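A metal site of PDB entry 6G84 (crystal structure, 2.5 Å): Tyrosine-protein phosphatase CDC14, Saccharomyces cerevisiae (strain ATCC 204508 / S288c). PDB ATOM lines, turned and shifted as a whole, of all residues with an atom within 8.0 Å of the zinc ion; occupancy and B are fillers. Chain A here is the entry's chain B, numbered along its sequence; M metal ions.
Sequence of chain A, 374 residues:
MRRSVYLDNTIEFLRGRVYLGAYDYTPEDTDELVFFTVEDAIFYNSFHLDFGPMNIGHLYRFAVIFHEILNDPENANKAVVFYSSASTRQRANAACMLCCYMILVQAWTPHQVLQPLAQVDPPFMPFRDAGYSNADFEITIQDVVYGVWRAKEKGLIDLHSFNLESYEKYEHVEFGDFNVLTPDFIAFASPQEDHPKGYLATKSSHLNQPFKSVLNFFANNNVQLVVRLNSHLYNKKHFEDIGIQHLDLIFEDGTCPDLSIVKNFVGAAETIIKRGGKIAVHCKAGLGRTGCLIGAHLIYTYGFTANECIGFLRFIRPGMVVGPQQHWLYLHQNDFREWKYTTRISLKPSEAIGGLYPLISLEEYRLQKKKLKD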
ATOM      1  N   GLU A 193     -24.786 -11.837   5.209  1.00  0.00           N
ATOM      2  CA  GLU A 193     -23.630 -11.069   5.649  1.00  0.00           C
ATOM      3  C   GLU A 193     -24.026  -9.601   5.756  1.00  0.00           C
ATOM      4  O   GLU A 193     -25.041  -9.171   5.196  1.00  0.00           O
ATOM      5  CB  GLU A 193     -22.447 -11.224   4.701  1.00  0.00           C
ATOM      6  CG  GLU A 193     -22.535 -10.347   3.467  1.00  0.00           C
ATOM      7  CD  GLU A 193     -21.256 -10.351   2.643  1.00  0.00           C
ATOM      8  OE1 GLU A 193     -21.056 -11.302   1.859  1.00  0.00           O
ATOM      9  OE2 GLU A 193     -20.453  -9.403   2.794  1.00  0.00           O
ATOM     10  N   ASP A 194     -23.213  -8.843   6.477  1.00  0.00           N
ATOM     11  CA  ASP A 194     -23.319  -7.385   6.560  1.00  0.00           C
ATOM     12  C   ASP A 194     -22.069  -6.803   5.904  1.00  0.00           C
ATOM     13  O   ASP A 194     -21.056  -6.566   6.563  1.00  0.00           O
ATOM     14  CB  ASP A 194     -23.464  -6.928   8.011  1.00  0.00           C
ATOM     15  CG  ASP A 194     -24.912  -6.736   8.425  1.00  0.00           C
ATOM     16  OD1 ASP A 194     -25.684  -6.167   7.622  1.00  0.00           O
ATOM     17  OD2 ASP A 194     -25.271  -7.134   9.547  1.00  0.00           O
ATOM     18  N   HIS A 195     -22.153  -6.580   4.598  1.00  0.00           N
ATOM     19  CA  HIS A 195     -20.999  -6.148   3.819  1.00  0.00           C
ATOM     20  C   HIS A 195     -20.667  -4.690   4.107  1.00  0.00           C
ATOM     21  O   HIS A 195     -21.509  -3.818   3.842  1.00  0.00           O
ATOM     22  CB  HIS A 195     -21.274  -6.349   2.329  1.00  0.00           C
ATOM     23  CG  HIS A 195     -20.037  -6.321   1.479  1.00  0.00           C
ATOM     24  ND1 HIS A 195     -19.167  -7.384   1.410  1.00  0.00           N
ATOM     25  CD2 HIS A 195     -19.533  -5.360   0.668  1.00  0.00           C
ATOM     26  CE1 HIS A 195     -18.175  -7.079   0.584  1.00  0.00           C
ATOM     27  NE2 HIS A 195     -18.381  -5.860   0.126  1.00  0.00           N
ATOM     28  N   PRO A 196     -19.487  -4.387   4.639  1.00  0.00           N
ATOM     29  CA  PRO A 196     -19.122  -2.981   4.863  1.00  0.00           C
ATOM     30  C   PRO A 196     -18.755  -2.300   3.562  1.00  0.00           C
ATOM     31  O   PRO A 196     -18.583  -2.921   2.511  1.00  0.00           O
ATOM     32  CB  PRO A 196     -17.927  -3.078   5.821  1.00  0.00           C
ATOM     33  CG  PRO A 196     -17.311  -4.397   5.497  1.00  0.00           C
ATOM     34  CD  PRO A 196     -18.451  -5.313   5.120  1.00  0.00           C
ATOM     35  N   LEU A 200     -12.643  -2.181   5.607  1.00  0.00           N
ATOM     36  CA  LEU A 200     -13.013  -3.404   6.307  1.00  0.00           C
ATOM     37  C   LEU A 200     -13.547  -4.474   5.363  1.00  0.00           C
ATOM     38  O   LEU A 200     -13.551  -5.655   5.721  1.00  0.00           O
ATOM     39  CB  LEU A 200     -14.049  -3.105   7.391  1.00  0.00           C
ATOM     40  CG  LEU A 200     -14.026  -1.724   8.065  1.00  0.00           C
ATOM     41  CD1 LEU A 200     -14.939  -0.739   7.329  1.00  0.00           C
ATOM     42  CD2 LEU A 200     -14.424  -1.832   9.530  1.00  0.00           C
ATOM     43  N   ALA A 201     -13.999  -4.097   4.171  1.00  0.00           N
ATOM     44  CA  ALA A 201     -14.551  -5.029   3.194  1.00  0.00           C
ATOM     45  C   ALA A 201     -13.484  -5.759   2.400  1.00  0.00           C
ATOM     46  O   ALA A 201     -13.804  -6.346   1.355  1.00  0.00           O
ATOM     47  CB  ALA A 201     -15.501  -4.291   2.249  1.00  0.00           C
ATOM     48  N   THR A 202     -12.238  -5.755   2.855  1.00  0.00           N
ATOM     49  CA  THR A 202     -11.156  -6.449   2.169  1.00  0.00           C
ATOM     50  C   THR A 202     -10.591  -7.627   2.953  1.00  0.00           C
ATOM     51  O   THR A 202      -9.766  -8.367   2.410  1.00  0.00           O
ATOM     52  CB  THR A 202     -10.015  -5.467   1.847  1.00  0.00           C
ATOM     53  N   LYS A 203     -11.004  -7.809   4.206  1.00  0.00           N
ATOM     54  CA  LYS A 203     -10.528  -8.897   5.046  1.00  0.00           C
ATOM     55  C   LYS A 203     -11.687  -9.807   5.412  1.00  0.00           C
ATOM     56  O   LYS A 203     -12.834  -9.365   5.538  1.00  0.00           O
ATOM     57  CB  LYS A 203      -9.854  -8.355   6.322  1.00  0.00           C
ATOM     58  N   SER A 204     -11.377 -11.094   5.595  1.00  0.00           N
ATOM     59  CA  SER A 204     -12.378 -12.086   5.977  1.00  0.00           C
ATOM     60  C   SER A 204     -12.568 -12.087   7.497  1.00  0.00           C
ATOM     61  O   SER A 204     -12.287 -13.049   8.198  1.00  0.00           O
ATOM     62  CB  SER A 204     -11.966 -13.469   5.472  1.00  0.00           C
ATOM     63  OG  SER A 204     -10.744 -13.886   6.051  1.00  0.00           O
ATOM     64  N   SER A 205     -13.072 -10.951   7.995  1.00  0.00           N
ATOM     65  CA  SER A 205     -13.356 -10.779   9.405  1.00  0.00           C
ATOM     66  C   SER A 205     -14.821 -10.498   9.705  1.00  0.00           C
ATOM     67  O   SER A 205     -15.276 -10.824  10.808  1.00  0.00           O
ATOM     68  CB  SER A 205     -12.507  -9.639   9.999  1.00  0.00           C
ATOM     69  OG  SER A 205     -12.709  -8.439   9.272  1.00  0.00           O
ATOM     70  N   HIS A 206     -15.561  -9.905   8.775  1.00  0.00           N
ATOM     71  CA  HIS A 206     -16.987  -9.676   8.943  1.00  0.00           C
ATOM     72  C   HIS A 206     -17.839 -10.869   8.519  1.00  0.00           C
ATOM     73  O   HIS A 206     -19.037 -10.875   8.793  1.00  0.00           O
ATOM     74  CB  HIS A 206     -17.424  -8.426   8.164  1.00  0.00           C
ATOM     75  CG  HIS A 206     -17.376  -8.607   6.674  1.00  0.00           C
ATOM     76  ND1 HIS A 206     -16.210  -8.533   5.950  1.00  0.00           N
ATOM     77  CD2 HIS A 206     -18.369  -8.842   5.784  1.00  0.00           C
ATOM     78  CE1 HIS A 206     -16.484  -8.725   4.670  1.00  0.00           C
ATOM     79  NE2 HIS A 206     -17.777  -8.915   4.548  1.00  0.00           N
ATOM     80  N   LEU A 207     -17.241 -11.856   7.853  1.00  0.00           N
ATOM     81  CA  LEU A 207     -17.971 -13.049   7.447  1.00  0.00           C
ATOM     82  C   LEU A 207     -18.166 -13.959   8.652  1.00  0.00           C
ATOM     83  O   LEU A 207     -17.218 -14.272   9.369  1.00  0.00           O
ATOM     84  CB  LEU A 207     -17.206 -13.787   6.353  1.00  0.00           C
ATOM     85  CG  LEU A 207     -16.839 -12.966   5.110  1.00  0.00           C
ATOM     86  CD1 LEU A 207     -15.993 -13.802   4.161  1.00  0.00           C
ATOM     87  CD2 LEU A 207     -18.085 -12.463   4.413  1.00  0.00           C
ATOM     88  N   PHE A 211     -20.867 -18.733   6.747  1.00  0.00           N
ATOM     89  CA  PHE A 211     -20.371 -18.265   5.460  1.00  0.00           C
ATOM     90  C   PHE A 211     -18.968 -18.809   5.200  1.00  0.00           C
ATOM     91  O   PHE A 211     -18.676 -19.308   4.104  1.00  0.00           O
ATOM     92  CB  PHE A 211     -20.387 -16.740   5.410  1.00  0.00           C
ATOM     93  CG  PHE A 211     -20.497 -16.168   4.017  1.00  0.00           C
ATOM     94  CD1 PHE A 211     -20.308 -16.966   2.896  1.00  0.00           C
ATOM     95  CD2 PHE A 211     -20.795 -14.829   3.831  1.00  0.00           C
ATOM     96  CE1 PHE A 211     -20.414 -16.445   1.620  1.00  0.00           C
ATOM     97  CE2 PHE A 211     -20.898 -14.294   2.559  1.00  0.00           C
ATOM     98  CZ  PHE A 211     -20.713 -15.105   1.456  1.00  0.00           C
ATOM     99  N   TYR A 234     -26.122 -11.290   0.196  1.00  0.00           N
ATOM    100  CA  TYR A 234     -24.678 -11.277   0.388  1.00  0.00           C
ATOM    101  C   TYR A 234     -24.037 -10.704  -0.867  1.00  0.00           C
ATOM    102  O   TYR A 234     -24.693 -10.480  -1.881  1.00  0.00           O
ATOM    103  CB  TYR A 234     -24.139 -12.684   0.694  1.00  0.00           C
ATOM    104  CG  TYR A 234     -24.315 -13.653  -0.453  1.00  0.00           C
ATOM    105  CD1 TYR A 234     -25.518 -14.344  -0.632  1.00  0.00           C
ATOM    106  CD2 TYR A 234     -23.284 -13.902  -1.353  1.00  0.00           C
ATOM    107  CE1 TYR A 234     -25.675 -15.230  -1.679  1.00  0.00           C
ATOM    108  CE2 TYR A 234     -23.441 -14.788  -2.400  1.00  0.00           C
ATOM    109  CZ  TYR A 234     -24.636 -15.451  -2.556  1.00  0.00           C
ATOM    110  OH  TYR A 234     -24.798 -16.339  -3.594  1.00  0.00           O
ATOM    111  N   ASN A 235     -22.724 -10.482  -0.783  1.00  0.00           N
ATOM    112  CA  ASN A 235     -21.962  -9.985  -1.913  1.00  0.00           C
ATOM    113  C   ASN A 235     -21.338 -11.155  -2.658  1.00  0.00           C
ATOM    114  O   ASN A 235     -20.678 -12.001  -2.065  1.00  0.00           O
ATOM    115  CB  ASN A 235     -20.875  -9.014  -1.445  1.00  0.00           C
ATOM    116  CG  ASN A 235     -20.385  -8.119  -2.558  1.00  0.00           C
ATOM    117  OD1 ASN A 235     -19.609  -8.532  -3.414  1.00  0.00           O
ATOM    118  ND2 ASN A 235     -20.841  -6.860  -2.559  1.00  0.00           N
ATOM    119  N   LYS A 236     -21.566 -11.197  -3.979  1.00  0.00           N
ATOM    120  CA  LYS A 236     -21.114 -12.329  -4.781  1.00  0.00           C
ATOM    121  C   LYS A 236     -19.602 -12.350  -4.979  1.00  0.00           C
ATOM    122  O   LYS A 236     -19.073 -13.368  -5.458  1.00  0.00           O
ATOM    123  CB  LYS A 236     -21.807 -12.334  -6.139  1.00  0.00           C
ATOM    124  CG  LYS A 236     -21.416 -11.187  -7.044  1.00  0.00           C
ATOM    125  CD  LYS A 236     -22.091 -11.297  -8.396  1.00  0.00           C
ATOM    126  CE  LYS A 236     -21.622 -10.212  -9.344  1.00  0.00           C
ATOM    127  NZ  LYS A 236     -20.148 -10.279  -9.585  1.00  0.00           N
ATOM    128  N   LYS A 237     -18.890 -11.273  -4.646  1.00  0.00           N
ATOM    129  CA  LYS A 237     -17.449 -11.232  -4.854  1.00  0.00           C
ATOM    130  C   LYS A 237     -16.707 -12.239  -3.981  1.00  0.00           C
ATOM    131  O   LYS A 237     -15.601 -12.643  -4.338  1.00  0.00           O
ATOM    132  CB  LYS A 237     -16.914  -9.821  -4.587  1.00  0.00           C
ATOM    133  N   HIS A 238     -17.297 -12.639  -2.853  1.00  0.00           N
ATOM    134  CA  HIS A 238     -16.639 -13.625  -1.995  1.00  0.00           C
ATOM    135  C   HIS A 238     -16.561 -14.995  -2.672  1.00  0.00           C
ATOM    136  O   HIS A 238     -15.652 -15.782  -2.361  1.00  0.00           O
ATOM    137  CB  HIS A 238     -17.377 -13.733  -0.662  1.00  0.00           C
ATOM    138  CG  HIS A 238     -17.380 -12.455   0.123  1.00  0.00           C
ATOM    139  ND1 HIS A 238     -16.342 -12.082   0.945  1.00  0.00           N
ATOM    140  CD2 HIS A 238     -18.306 -11.479   0.210  1.00  0.00           C
ATOM    141  CE1 HIS A 238     -16.623 -10.922   1.508  1.00  0.00           C
ATOM    142  NE2 HIS A 238     -17.808 -10.524   1.070  1.00  0.00           N
HETATM  143 ZN    ZN M   1     -18.465  -9.195   2.544  1.00  0.00          ZN
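The backbone NH (N) of Asn 235 sits at hydrogen-bond distance from the side-chain carboxylate (OE1) of Glu 193 (3.2 Å).
Leu 207 touches the zinc ion (CD2 to ZN, 3.8 Å). The nearest printed residue that does not touch the zinc ion is Pro 196 (4.7 Å).
The zinc ion is bound by OE2 of Glu 193, NE2 of His 238, NE2 of His 206 and ND1 of His 195. The zinc ion has four donor atoms within binding distance.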
